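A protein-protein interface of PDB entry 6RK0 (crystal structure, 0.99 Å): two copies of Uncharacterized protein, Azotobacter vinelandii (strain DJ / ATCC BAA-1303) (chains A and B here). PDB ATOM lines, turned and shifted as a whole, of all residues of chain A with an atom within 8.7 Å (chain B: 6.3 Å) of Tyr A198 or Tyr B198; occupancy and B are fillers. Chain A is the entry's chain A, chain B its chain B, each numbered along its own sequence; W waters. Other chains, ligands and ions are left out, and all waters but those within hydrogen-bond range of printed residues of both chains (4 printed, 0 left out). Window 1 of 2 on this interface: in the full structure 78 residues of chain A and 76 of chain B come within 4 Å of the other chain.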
ATOM      1  N   ALA A  41      -5.806 -13.743 -11.634  1.00  0.00           N
ATOM      2  CA  ALA A  41      -7.006 -13.806 -12.446  1.00  0.00           C
ATOM      3  C   ALA A  41      -7.746 -12.487 -12.587  1.00  0.00           C
ATOM      4  O   ALA A  41      -8.646 -12.401 -13.433  1.00  0.00           O
ATOM      5  CB  ALA A  41      -7.959 -14.853 -11.903  1.00  0.00           C
ATOM      6  N   THR A  42      -7.414 -11.470 -11.795  1.00  0.00           N
ATOM      7  CA  THR A  42      -8.240 -10.277 -11.717  1.00  0.00           C
ATOM      8  C   THR A  42      -7.388  -9.108 -11.254  1.00  0.00           C
ATOM      9  O   THR A  42      -6.468  -9.300 -10.468  1.00  0.00           O
ATOM     10  CB  THR A  42      -9.420 -10.509 -10.759  1.00  0.00           C
ATOM     11  OG1 THR A  42     -10.182  -9.299 -10.719  1.00  0.00           O
ATOM     12  CG2 THR A  42      -8.984 -10.912  -9.356  1.00  0.00           C
ATOM     13  N   PRO A  43      -7.726  -7.883 -11.672  1.00  0.00           N
ATOM     14  CA  PRO A  43      -7.005  -6.705 -11.189  1.00  0.00           C
ATOM     15  C   PRO A  43      -7.657  -6.035 -10.001  1.00  0.00           C
ATOM     16  O   PRO A  43      -7.068  -5.066  -9.501  1.00  0.00           O
ATOM     17  CB  PRO A  43      -7.067  -5.769 -12.395  1.00  0.00           C
ATOM     18  CG  PRO A  43      -8.423  -6.063 -12.984  1.00  0.00           C
ATOM     19  CD  PRO A  43      -8.601  -7.553 -12.813  1.00  0.00           C
ATOM     20  N   LEU A  44      -8.847  -6.470  -9.571  1.00  0.00           N
ATOM     21  CA  LEU A  44      -9.626  -5.685  -8.612  1.00  0.00           C
ATOM     22  C   LEU A  44      -9.549  -6.257  -7.198  1.00  0.00           C
ATOM     23  O   LEU A  44     -10.026  -7.390  -6.948  1.00  0.00           O
ATOM     24  CB  LEU A  44     -11.089  -5.596  -9.058  1.00  0.00           C
ATOM     25  CG  LEU A  44     -12.037  -4.836  -8.133  1.00  0.00           C
ATOM     26  CD1 LEU A  44     -11.590  -3.394  -7.935  1.00  0.00           C
ATOM     27  CD2 LEU A  44     -13.473  -4.911  -8.634  1.00  0.00           C
ATOM     28  N   ALA A  45      -9.030  -5.440  -6.272  1.00  0.00           N
ATOM     29  CA  ALA A  45      -8.951  -5.761  -4.844  1.00  0.00           C
ATOM     30  C   ALA A  45      -9.801  -4.795  -4.040  1.00  0.00           C
ATOM     31  O   ALA A  45     -10.193  -3.725  -4.528  1.00  0.00           O
ATOM     32  CB  ALA A  45      -7.506  -5.674  -4.368  1.00  0.00           C
ATOM     33  N   HIS A  46      -9.987  -5.145  -2.775  1.00  0.00           N
ATOM     34  CA  HIS A  46     -10.627  -4.281  -1.796  1.00  0.00           C
ATOM     35  C   HIS A  46      -9.742  -4.266  -0.561  1.00  0.00           C
ATOM     36  O   HIS A  46      -9.514  -5.303   0.069  1.00  0.00           O
ATOM     37  CB  HIS A  46     -12.046  -4.790  -1.462  1.00  0.00           C
ATOM     38  CG  HIS A  46     -12.998  -4.604  -2.594  1.00  0.00           C
ATOM     39  ND1 HIS A  46     -13.067  -5.460  -3.669  1.00  0.00           N
ATOM     40  CD2 HIS A  46     -13.856  -3.586  -2.880  1.00  0.00           C
ATOM     41  CE1 HIS A  46     -13.924  -4.955  -4.549  1.00  0.00           C
ATOM     42  NE2 HIS A  46     -14.427  -3.827  -4.100  1.00  0.00           N
ATOM     43  N   PHE A  61      -7.086  -1.196  -7.952  1.00  0.00           N
ATOM     44  CA  PHE A  61      -6.375  -2.177  -8.747  1.00  0.00           C
ATOM     45  C   PHE A  61      -5.141  -2.673  -8.022  1.00  0.00           C
ATOM     46  O   PHE A  61      -4.603  -2.008  -7.129  1.00  0.00           O
ATOM     47  CB  PHE A  61      -6.007  -1.603 -10.103  1.00  0.00           C
ATOM     48  CG  PHE A  61      -7.194  -1.412 -10.967  1.00  0.00           C
ATOM     49  CD1 PHE A  61      -7.550  -0.170 -11.386  1.00  0.00           C
ATOM     50  CD2 PHE A  61      -8.088  -2.455 -11.173  1.00  0.00           C
ATOM     51  CE1 PHE A  61      -8.648   0.029 -12.185  1.00  0.00           C
ATOM     52  CE2 PHE A  61      -9.234  -2.266 -11.953  1.00  0.00           C
ATOM     53  CZ  PHE A  61      -9.491  -0.998 -12.455  1.00  0.00           C
ATOM     54  N   SER A  93     -11.796 -10.917  -4.534  1.00  0.00           N
ATOM     55  CA  SER A  93     -12.920 -11.827  -4.733  1.00  0.00           C
ATOM     56  C   SER A  93     -13.268 -11.933  -6.212  1.00  0.00           C
ATOM     57  O   SER A  93     -13.230 -10.951  -6.957  1.00  0.00           O
ATOM     58  CB  SER A  93     -14.160 -11.431  -3.951  1.00  0.00           C
ATOM     59  OG  SER A  93     -14.555 -10.151  -4.244  1.00  0.00           O
ATOM     60  N   LEU A  94     -13.714 -13.123  -6.610  1.00  0.00           N
ATOM     61  CA  LEU A  94     -14.326 -13.390  -7.910  1.00  0.00           C
ATOM     62  C   LEU A  94     -15.595 -14.179  -7.696  1.00  0.00           C
ATOM     63  O   LEU A  94     -15.570 -15.284  -7.131  1.00  0.00           O
ATOM     64  CB  LEU A  94     -13.394 -14.104  -8.878  1.00  0.00           C
ATOM     65  CG  LEU A  94     -12.267 -13.240  -9.431  1.00  0.00           C
ATOM     66  CD1 LEU A  94     -11.220 -14.094 -10.110  1.00  0.00           C
ATOM     67  CD2 LEU A  94     -12.800 -12.156 -10.369  1.00  0.00           C
ATOM     68  N   LEU A  95     -16.709 -13.641  -8.185  1.00  0.00           N
ATOM     69  CA  LEU A  95     -18.008 -14.320  -8.177  1.00  0.00           C
ATOM     70  C   LEU A  95     -18.132 -15.150  -9.447  1.00  0.00           C
ATOM     71  O   LEU A  95     -18.060 -14.612 -10.557  1.00  0.00           O
ATOM     72  CB  LEU A  95     -19.114 -13.274  -8.068  1.00  0.00           C
ATOM     73  CG  LEU A  95     -20.528 -13.802  -8.194  1.00  0.00           C
ATOM     74  CD1 LEU A  95     -20.859 -14.869  -7.117  1.00  0.00           C
ATOM     75  CD2 LEU A  95     -21.508 -12.629  -8.108  1.00  0.00           C
ATOM     76  N   ASP A  96     -18.328 -16.470  -9.294  1.00  0.00           N
ATOM     77  CA  ASP A  96     -18.297 -17.403 -10.412  1.00  0.00           C
ATOM     78  C   ASP A  96     -19.648 -18.051 -10.734  1.00  0.00           C
ATOM     79  O   ASP A  96     -19.775 -18.680 -11.778  1.00  0.00           O
ATOM     80  CB  ASP A  96     -17.254 -18.500 -10.191  1.00  0.00           C
ATOM     81  CG  ASP A  96     -15.831 -17.951 -10.033  1.00  0.00           C
ATOM     82  OD1 ASP A  96     -15.510 -16.955 -10.748  1.00  0.00           O
ATOM     83  OD2 ASP A  96     -15.033 -18.511  -9.242  1.00  0.00           O
ATOM     84  N   GLY A  97     -20.655 -17.937  -9.862  1.00  0.00           N
ATOM     85  CA  GLY A  97     -21.958 -18.490 -10.190  1.00  0.00           C
ATOM     86  C   GLY A  97     -22.899 -18.359  -9.022  1.00  0.00           C
ATOM     87  O   GLY A  97     -22.471 -18.230  -7.879  1.00  0.00           O
ATOM     88  N   ARG A 112     -14.082 -17.599  -5.959  1.00  0.00           N
ATOM     89  CA  ARG A 112     -12.695 -17.686  -5.497  1.00  0.00           C
ATOM     90  C   ARG A 112     -12.414 -16.445  -4.683  1.00  0.00           C
ATOM     91  O   ARG A 112     -12.728 -15.338  -5.143  1.00  0.00           O
ATOM     92  CB  ARG A 112     -11.723 -17.736  -6.693  1.00  0.00           C
ATOM     93  CG  ARG A 112     -11.827 -19.004  -7.515  1.00  0.00           C
ATOM     94  CD  ARG A 112     -11.252 -18.822  -8.911  1.00  0.00           C
ATOM     95  NE  ARG A 112     -12.177 -18.046  -9.723  1.00  0.00           N
ATOM     96  CZ  ARG A 112     -11.861 -17.555 -10.917  1.00  0.00           C
ATOM     97  NH1 ARG A 112     -10.603 -17.613 -11.363  1.00  0.00           N
ATOM     98  NH2 ARG A 112     -12.782 -16.986 -11.666  1.00  0.00           N
ATOM     99  N   PRO A 195     -23.901 -19.797 -14.122  1.00  0.00           N
ATOM    100  CA  PRO A 195     -22.523 -19.304 -14.159  1.00  0.00           C
ATOM    101  C   PRO A 195     -22.482 -17.807 -14.371  1.00  0.00           C
ATOM    102  O   PRO A 195     -23.307 -17.237 -15.092  1.00  0.00           O
ATOM    103  CB  PRO A 195     -21.892 -20.032 -15.346  1.00  0.00           C
ATOM    104  CG  PRO A 195     -22.822 -21.212 -15.634  1.00  0.00           C
ATOM    105  CD  PRO A 195     -24.194 -20.694 -15.244  1.00  0.00           C
ATOM    106  N   ILE A 196     -21.463 -17.179 -13.762  1.00  0.00           N
ATOM    107  CA  ILE A 196     -21.231 -15.722 -13.838  1.00  0.00           C
ATOM    108  C   ILE A 196     -19.755 -15.544 -14.165  1.00  0.00           C
ATOM    109  O   ILE A 196     -18.909 -16.230 -13.578  1.00  0.00           O
ATOM    110  CB  ILE A 196     -21.540 -15.068 -12.470  1.00  0.00           C
ATOM    111  CG1 ILE A 196     -23.019 -15.221 -12.111  1.00  0.00           C
ATOM    112  CG2 ILE A 196     -21.058 -13.598 -12.424  1.00  0.00           C
ATOM    113  CD1 ILE A 196     -23.344 -14.924 -10.645  1.00  0.00           C
ATOM    114  N   ARG A 197     -19.440 -14.582 -15.033  1.00  0.00           N
ATOM    115  CA  ARG A 197     -18.046 -14.252 -15.283  1.00  0.00           C
ATOM    116  C   ARG A 197     -17.942 -12.809 -15.746  1.00  0.00           C
ATOM    117  O   ARG A 197     -18.907 -12.210 -16.222  1.00  0.00           O
ATOM    118  CB  ARG A 197     -17.430 -15.173 -16.337  1.00  0.00           C
ATOM    119  CG  ARG A 197     -18.067 -15.023 -17.686  1.00  0.00           C
ATOM    120  CD  ARG A 197     -17.480 -16.000 -18.654  1.00  0.00           C
ATOM    121  NE  ARG A 197     -18.069 -15.844 -19.965  1.00  0.00           N
ATOM    122  CZ  ARG A 197     -17.910 -16.717 -20.958  1.00  0.00           C
ATOM    123  NH1 ARG A 197     -17.167 -17.799 -20.781  1.00  0.00           N
ATOM    124  NH2 ARG A 197     -18.512 -16.526 -22.122  1.00  0.00           N
ATOM    125  N   TYR A 198     -16.722 -12.273 -15.675  1.00  0.00           N
ATOM    126  CA  TYR A 198     -16.459 -11.017 -16.371  1.00  0.00           C
ATOM    127  C   TYR A 198     -16.380 -11.258 -17.874  1.00  0.00           C
ATOM    128  O   TYR A 198     -15.875 -12.274 -18.343  1.00  0.00           O
ATOM    129  CB  TYR A 198     -15.143 -10.411 -15.892  1.00  0.00           C
ATOM    130  CG  TYR A 198     -15.228  -9.640 -14.611  1.00  0.00           C
ATOM    131  CD1 TYR A 198     -16.031  -8.501 -14.516  1.00  0.00           C
ATOM    132  CD2 TYR A 198     -14.496 -10.012 -13.490  1.00  0.00           C
ATOM    133  CE1 TYR A 198     -16.105  -7.754 -13.352  1.00  0.00           C
ATOM    134  CE2 TYR A 198     -14.551  -9.271 -12.333  1.00  0.00           C
ATOM    135  CZ  TYR A 198     -15.347  -8.134 -12.251  1.00  0.00           C
ATOM    136  OH  TYR A 198     -15.389  -7.372 -11.108  1.00  0.00           O
ATOM    137  N   GLN A 199     -16.835 -10.254 -18.620  1.00  0.00           N
ATOM    138  CA  GLN A 199     -16.739 -10.202 -20.074  1.00  0.00           C
ATOM    139  C   GLN A 199     -16.103  -8.879 -20.471  1.00  0.00           C
ATOM    140  O   GLN A 199     -16.472  -7.826 -19.967  1.00  0.00           O
ATOM    141  CB  GLN A 199     -18.174 -10.284 -20.671  1.00  0.00           C
ATOM    142  CG  GLN A 199     -18.197 -10.235 -22.190  1.00  0.00           C
ATOM    143  CD  GLN A 199     -19.589 -10.358 -22.742  1.00  0.00           C
ATOM    144  OE1 GLN A 199     -20.552  -9.869 -22.143  1.00  0.00           O
ATOM    145  NE2 GLN A 199     -19.707 -11.001 -23.911  1.00  0.00           N
ATOM    146  N   VAL A 200     -15.182  -8.964 -21.402  1.00  0.00           N
ATOM    147  CA  VAL A 200     -14.544  -7.794 -21.972  1.00  0.00           C
ATOM    148  C   VAL A 200     -15.133  -7.595 -23.359  1.00  0.00           C
ATOM    149  O   VAL A 200     -15.298  -8.564 -24.108  1.00  0.00           O
ATOM    150  CB  VAL A 200     -13.033  -8.040 -22.026  1.00  0.00           C
ATOM    151  CG1 VAL A 200     -12.361  -7.078 -22.831  1.00  0.00           C
ATOM    152  CG2 VAL A 200     -12.464  -8.046 -20.685  1.00  0.00           C
ATOM    153  N   LEU A 201     -15.520  -6.365 -23.682  1.00  0.00           N
ATOM    154  CA  LEU A 201     -16.118  -6.049 -24.966  1.00  0.00           C
ATOM    155  C   LEU A 201     -15.082  -5.414 -25.877  1.00  0.00           C
ATOM    156  O   LEU A 201     -14.004  -5.012 -25.423  1.00  0.00           O
ATOM    157  CB  LEU A 201     -17.320  -5.127 -24.752  1.00  0.00           C
ATOM    158  CG  LEU A 201     -18.452  -5.734 -23.908  1.00  0.00           C
ATOM    159  CD1 LEU A 201     -19.571  -4.724 -23.743  1.00  0.00           C
ATOM    160  CD2 LEU A 201     -18.984  -7.032 -24.505  1.00  0.00           C
ATOM    161  N   PHE A 222      -5.844  -7.696 -23.169  1.00  0.00           N
ATOM    162  CA  PHE A 222      -6.332  -7.448 -21.819  1.00  0.00           C
ATOM    163  C   PHE A 222      -7.503  -8.389 -21.531  1.00  0.00           C
ATOM    164  O   PHE A 222      -8.427  -8.504 -22.341  1.00  0.00           O
ATOM    165  CB  PHE A 222      -6.760  -5.995 -21.658  1.00  0.00           C
ATOM    166  CG  PHE A 222      -7.545  -5.762 -20.399  1.00  0.00           C
ATOM    167  CD1 PHE A 222      -6.918  -5.714 -19.153  1.00  0.00           C
ATOM    168  CD2 PHE A 222      -8.918  -5.699 -20.439  1.00  0.00           C
ATOM    169  CE1 PHE A 222      -7.646  -5.569 -17.994  1.00  0.00           C
ATOM    170  CE2 PHE A 222      -9.645  -5.526 -19.266  1.00  0.00           C
ATOM    171  CZ  PHE A 222      -9.001  -5.470 -18.062  1.00  0.00           C
ATOM    172  N   ARG A 223      -7.484  -9.016 -20.354  1.00  0.00           N
ATOM    173  CA  ARG A 223      -8.543  -9.943 -19.950  1.00  0.00           C
ATOM    174  C   ARG A 223      -8.640  -9.923 -18.438  1.00  0.00           C
ATOM    175  O   ARG A 223      -7.705  -9.489 -17.763  1.00  0.00           O
ATOM    176  CB  ARG A 223      -8.254 -11.368 -20.454  1.00  0.00           C
ATOM    177  CG  ARG A 223      -6.888 -11.923 -20.053  1.00  0.00           C
ATOM    178  CD  ARG A 223      -6.877 -12.624 -18.692  1.00  0.00           C
ATOM    179  NE  ARG A 223      -7.962 -13.615 -18.612  1.00  0.00           N
ATOM    180  CZ  ARG A 223      -8.597 -13.994 -17.499  1.00  0.00           C
ATOM    181  NH1 ARG A 223      -8.219 -13.582 -16.295  1.00  0.00           N
ATOM    182  NH2 ARG A 223      -9.608 -14.849 -17.602  1.00  0.00           N
ATOM    183  N   LEU A 224      -9.769 -10.416 -17.910  1.00  0.00           N
ATOM    184  CA  LEU A 224      -9.897 -10.536 -16.460  1.00  0.00           C
ATOM    185  C   LEU A 224     -10.954 -11.587 -16.159  1.00  0.00           C
ATOM    186  O   LEU A 224     -11.841 -11.877 -16.971  1.00  0.00           O
ATOM    187  CB  LEU A 224     -10.253  -9.216 -15.736  1.00  0.00           C
ATOM    188  CG  LEU A 224     -11.708  -8.720 -15.828  1.00  0.00           C
ATOM    189  CD1 LEU A 224     -11.904  -7.551 -14.884  1.00  0.00           C
ATOM    190  CD2 LEU A 224     -12.114  -8.340 -17.249  1.00  0.00           C
ATOM    191  N   GLY A 225     -10.912 -12.060 -14.911  1.00  0.00           N
ATOM    192  CA  GLY A 225     -11.936 -12.925 -14.370  1.00  0.00           C
ATOM    193  C   GLY A 225     -11.594 -14.387 -14.410  1.00  0.00           C
ATOM    194  O   GLY A 225     -10.514 -14.778 -14.915  1.00  0.00           O
ATOM    195  OXT GLY A 225     -12.468 -15.138 -13.902  1.00  0.00           O
ATOM    196  N   THR B  42     -26.211  -4.918  -8.394  1.00  0.00           N
ATOM    197  CA  THR B  42     -25.281  -6.007  -8.118  1.00  0.00           C
ATOM    198  C   THR B  42     -25.593  -6.580  -6.750  1.00  0.00           C
ATOM    199  O   THR B  42     -26.009  -5.841  -5.857  1.00  0.00           O
ATOM    200  CB  THR B  42     -23.833  -5.475  -8.165  1.00  0.00           C
ATOM    201  OG1 THR B  42     -22.952  -6.559  -7.882  1.00  0.00           O
ATOM    202  CG2 THR B  42     -23.575  -4.331  -7.230  1.00  0.00           C
ATOM    203  N   PRO B  43     -25.300  -7.869  -6.539  1.00  0.00           N
ATOM    204  CA  PRO B  43     -25.486  -8.485  -5.225  1.00  0.00           C
ATOM    205  C   PRO B  43     -24.242  -8.480  -4.369  1.00  0.00           C
ATOM    206  O   PRO B  43     -24.335  -8.928  -3.217  1.00  0.00           O
ATOM    207  CB  PRO B  43     -25.852  -9.941  -5.572  1.00  0.00           C
ATOM    208  CG  PRO B  43     -25.024 -10.212  -6.798  1.00  0.00           C
ATOM    209  CD  PRO B  43     -25.068  -8.885  -7.584  1.00  0.00           C
ATOM    210  N   LEU B  44     -23.072  -8.094  -4.892  1.00  0.00           N
ATOM    211  CA  LEU B  44     -21.812  -8.349  -4.210  1.00  0.00           C
ATOM    212  C   LEU B  44     -21.270  -7.105  -3.508  1.00  0.00           C
ATOM    213  O   LEU B  44     -20.929  -6.097  -4.175  1.00  0.00           O
ATOM    214  CB  LEU B  44     -20.766  -8.877  -5.187  1.00  0.00           C
ATOM    215  CG  LEU B  44     -19.393  -9.175  -4.574  1.00  0.00           C
ATOM    216  CD1 LEU B  44     -19.438 -10.207  -3.479  1.00  0.00           C
ATOM    217  CD2 LEU B  44     -18.407  -9.608  -5.683  1.00  0.00           C
ATOM    218  N   SER B  93     -18.776  -2.161  -5.305  1.00  0.00           N
ATOM    219  CA  SER B  93     -18.073  -1.666  -6.484  1.00  0.00           C
ATOM    220  C   SER B  93     -18.465  -2.463  -7.723  1.00  0.00           C
ATOM    221  O   SER B  93     -18.681  -3.674  -7.665  1.00  0.00           O
ATOM    222  CB  SER B  93     -16.567  -1.711  -6.291  1.00  0.00           C
ATOM    223  OG  SER B  93     -16.136  -3.065  -6.096  1.00  0.00           O
ATOM    224  N   LEU B  94     -18.513  -1.754  -8.853  1.00  0.00           N
ATOM    225  CA  LEU B  94     -18.669  -2.343 -10.168  1.00  0.00           C
ATOM    226  C   LEU B  94     -17.609  -1.761 -11.087  1.00  0.00           C
ATOM    227  O   LEU B  94     -17.532  -0.541 -11.264  1.00  0.00           O
ATOM    228  CB  LEU B  94     -20.053  -2.117 -10.752  1.00  0.00           C
ATOM    229  CG  LEU B  94     -21.157  -2.931 -10.110  1.00  0.00           C
ATOM    230  CD1 LEU B  94     -22.525  -2.438 -10.548  1.00  0.00           C
ATOM    231  CD2 LEU B  94     -21.009  -4.435 -10.441  1.00  0.00           C
ATOM    232  N   LEU B  95     -16.805  -2.639 -11.662  1.00  0.00           N
ATOM    233  CA  LEU B  95     -15.806  -2.270 -12.658  1.00  0.00           C
ATOM    234  C   LEU B  95     -16.454  -2.290 -14.033  1.00  0.00           C
ATOM    235  O   LEU B  95     -16.949  -3.322 -14.494  1.00  0.00           O
ATOM    236  CB  LEU B  95     -14.641  -3.246 -12.584  1.00  0.00           C
ATOM    237  CG  LEU B  95     -13.542  -3.086 -13.627  1.00  0.00           C
ATOM    238  CD1 LEU B  95     -12.921  -1.675 -13.621  1.00  0.00           C
ATOM    239  CD2 LEU B  95     -12.507  -4.186 -13.407  1.00  0.00           C
ATOM    240  N   ILE B 196     -16.041  -3.406 -19.706  1.00  0.00           N
ATOM    241  CA  ILE B 196     -16.060  -4.611 -18.877  1.00  0.00           C
ATOM    242  C   ILE B 196     -17.442  -4.736 -18.268  1.00  0.00           C
ATOM    243  O   ILE B 196     -18.007  -3.726 -17.837  1.00  0.00           O
ATOM    244  CB  ILE B 196     -15.023  -4.493 -17.744  1.00  0.00           C
ATOM    245  CG1 ILE B 196     -13.601  -4.424 -18.325  1.00  0.00           C
ATOM    246  CG2 ILE B 196     -15.150  -5.614 -16.706  1.00  0.00           C
ATOM    247  CD1 ILE B 196     -12.560  -3.925 -17.334  1.00  0.00           C
ATOM    248  N   ARG B 197     -17.995  -5.956 -18.198  1.00  0.00           N
ATOM    249  CA  ARG B 197     -19.267  -6.140 -17.514  1.00  0.00           C
ATOM    250  C   ARG B 197     -19.359  -7.562 -17.008  1.00  0.00           C
ATOM    251  O   ARG B 197     -18.657  -8.458 -17.481  1.00  0.00           O
ATOM    252  CB  ARG B 197     -20.456  -5.852 -18.415  1.00  0.00           C
ATOM    253  CG  ARG B 197     -20.603  -6.814 -19.582  1.00  0.00           C
ATOM    254  CD  ARG B 197     -21.747  -6.414 -20.452  1.00  0.00           C
ATOM    255  NE  ARG B 197     -21.910  -7.380 -21.511  1.00  0.00           N
ATOM    256  CZ  ARG B 197     -22.671  -7.175 -22.580  1.00  0.00           C
ATOM    257  NH1 ARG B 197     -23.332  -6.028 -22.713  1.00  0.00           N
ATOM    258  NH2 ARG B 197     -22.750  -8.108 -23.514  1.00  0.00           N
ATOM    259  N   TYR B 198     -20.268  -7.787 -16.060  1.00  0.00           N
ATOM    260  CA  TYR B 198     -20.654  -9.166 -15.739  1.00  0.00           C
ATOM    261  C   TYR B 198     -21.497  -9.762 -16.857  1.00  0.00           C
ATOM    262  O   TYR B 198     -22.345  -9.081 -17.480  1.00  0.00           O
ATOM    263  CB  TYR B 198     -21.463  -9.194 -14.444  1.00  0.00           C
ATOM    264  CG  TYR B 198     -20.615  -9.160 -13.195  1.00  0.00           C
ATOM    265  CD1 TYR B 198     -19.686 -10.195 -12.923  1.00  0.00           C
ATOM    266  CD2 TYR B 198     -20.740  -8.153 -12.253  1.00  0.00           C
ATOM    267  CE1 TYR B 198     -18.932 -10.218 -11.737  1.00  0.00           C
ATOM    268  CE2 TYR B 198     -20.024  -8.174 -11.079  1.00  0.00           C
ATOM    269  CZ  TYR B 198     -19.108  -9.198 -10.827  1.00  0.00           C
ATOM    270  OH  TYR B 198     -18.404  -9.207  -9.654  1.00  0.00           O
ATOM    271  N   GLN B 199     -21.299 -11.058 -17.072  1.00  0.00           N
ATOM    272  CA  GLN B 199     -22.078 -11.861 -17.992  1.00  0.00           C
ATOM    273  C   GLN B 199     -22.621 -13.068 -17.222  1.00  0.00           C
ATOM    274  O   GLN B 199     -21.899 -13.721 -16.476  1.00  0.00           O
ATOM    275  CB  GLN B 199     -21.190 -12.354 -19.162  1.00  0.00           C
ATOM    276  CG  GLN B 199     -21.909 -13.227 -20.177  1.00  0.00           C
ATOM    277  CD  GLN B 199     -20.989 -13.646 -21.310  1.00  0.00           C
ATOM    278  OE1 GLN B 199     -19.786 -13.868 -21.088  1.00  0.00           O
ATOM    279  NE2 GLN B 199     -21.545 -13.799 -22.510  1.00  0.00           N
ATOM    280  N   VAL B 200     -23.898 -13.358 -17.446  1.00  0.00           N
ATOM    281  CA  VAL B 200     -24.555 -14.538 -16.924  1.00  0.00           C
ATOM    282  C   VAL B 200     -24.714 -15.538 -18.064  1.00  0.00           C
ATOM    283  O   VAL B 200     -25.105 -15.158 -19.175  1.00  0.00           O
ATOM    284  CB  VAL B 200     -25.910 -14.109 -16.344  1.00  0.00           C
ATOM    285  CG1 VAL B 200     -26.828 -15.235 -16.177  1.00  0.00           C
ATOM    286  CG2 VAL B 200     -25.740 -13.343 -15.075  1.00  0.00           C
ATOM    287  N   LEU B 224     -27.039  -9.434 -13.190  1.00  0.00           N
ATOM    288  CA  LEU B 224     -26.229  -8.587 -12.320  1.00  0.00           C
ATOM    289  C   LEU B 224     -25.331  -7.726 -13.183  1.00  0.00           C
ATOM    290  O   LEU B 224     -25.037  -8.066 -14.336  1.00  0.00           O
ATOM    291  CB  LEU B 224     -25.373  -9.358 -11.306  1.00  0.00           C
ATOM    292  CG  LEU B 224     -24.079 -10.038 -11.800  1.00  0.00           C
ATOM    293  CD1 LEU B 224     -23.275 -10.512 -10.619  1.00  0.00           C
ATOM    294  CD2 LEU B 224     -24.356 -11.166 -12.767  1.00  0.00           C
ATOM    295  N   GLY B 225     -24.846  -6.640 -12.559  1.00  0.00           N
ATOM    296  CA  GLY B 225     -23.842  -5.785 -13.155  1.00  0.00           C
ATOM    297  C   GLY B 225     -24.365  -4.559 -13.826  1.00  0.00           C
ATOM    298  O   GLY B 225     -23.511  -3.792 -14.324  1.00  0.00           O
ATOM    299  OXT GLY B 225     -25.617  -4.332 -13.842  1.00  0.00           O
HETATM  300  O   HOH W   1     -23.381 -10.352 -22.009  1.00  0.00           O
HETATM  301  O   HOH W   2     -17.342  -5.496 -10.910  1.00  0.00           O
HETATM  302  O   HOH W   3     -17.398 -13.579 -22.714  1.00  0.00           O
HETATM  303  O   HOH W   4     -16.330 -10.949  -9.472  1.00  0.00           O
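NE2 of His A46 is in hydrogen-bond range of OG of Ser B93 (2.7 Å).
The backbone NH (N) of Gln B199 lies within hydrogen-bond range of the backbone carbonyl oxygen (O) of Arg A197 (2.8 Å).
The backbone NH (N) of Gln A199 is in hydrogen-bond range of the backbone carbonyl oxygen (O) of Arg B197 (2.8 Å).
The backbone NH (N) of Ile A196 is in hydrogen-bond range of the backbone carbonyl oxygen (O) of Asp A96, 3.0 Å away.
Among the printed residues, merely in contact across the chains: Phe A61 with Leu B95 (3.7 Å), Leu A95 with Leu B224 (3.7 Å), Pro A195 with Val B200 (3.5 Å), Ile A196 with Tyr B198 (3.7 Å), Ile A196 with Gln B199 (3.4 Å), Arg A197 with Arg B197 (3.97 Å), Arg A197 with Tyr B198 (3.5 Å), Tyr A198 with Ile B196 (3.7 Å), Tyr A198 with Arg B197 (3.6 Å), Tyr A198 with Tyr B198 (3.8 Å), Gln A199 with Ile B196 (3.4 Å), Gln A199 with Gln B199 (3.6 Å), Phe A222 with Ile B196 (3.8 Å) and Leu A224 with Leu B95 (3.7 Å).
Tyr A198 touches just these residues of chain B: Ile B196, Arg B197 and Tyr B198.
Tyr B198 touches just these residues of chain A: Ile A196, Arg A197 and Tyr A198.
Of the printed residues of chain B, Leu A224 touches Leu B95.
Of the printed residues of chain B, Pro A195 touches Val B200.
Printed residues of chain B within 4 Å of His A46: Ser B93.
Printed residues of chain B within 4 Å of Phe A222: Ile B196 (3.8 Å).
The nearest printed residue of chain A that does not touch Ile B196 is Leu A224 (4.1 Å).
Of the 24 printed residues of chain A, 10 touch a printed residue of chain B.
Printed residues of chain A that touch a printed residue of chain B: His A46, Phe A61, Leu A95, Pro A195, Ile A196, Arg A197, Tyr A198, Gln A199, Phe A222 and Leu A224.
Of the 13 printed residues of chain B, 8 touch a printed residue of chain A.
Among the printed residues, no Asp or Glu carboxylate lies within 4 Å of a Lys or Arg side-chain nitrogen of the other chain.
Leu A95 touches Leu B224, and with the chains exchanged Leu A224 touches Leu B95.
Ile A196 touches Tyr B198, and with the chains exchanged Tyr A198 touches Ile B196.
Arg A197 touches Gln B199, and with the chains exchanged Gln A199 touches Arg B197.
Gln A199 touches its own counterpart, Gln B199.
Positions printed for both chains: 42, 43, 44, 93, 94, 95, 196, 197, 198, 199, 200, 224 and 225.
Of the 17 pairs that touch across the chains among the printed residues, 13 have their exchanged pair printed and touching as well.
Water W4 bridges the side-chain hydroxyl of Tyr B198 (2.7 Å) and the backbone NH of Leu A95 (3.0 Å).
Water W2 bridges OH of Tyr A198 (2.7 Å) and N of Leu B95 (3.0 Å).
Water W1 lies within hydrogen-bond range of the guanidinium group of Arg B197 (2.8 Å) and the side-chain amide oxygen of Gln A199 (2.9 Å).
Water W3 lies within hydrogen-bond range of OE1 of Gln B199 (2.9 Å) and NH2 of Arg A197 (3.2 Å).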
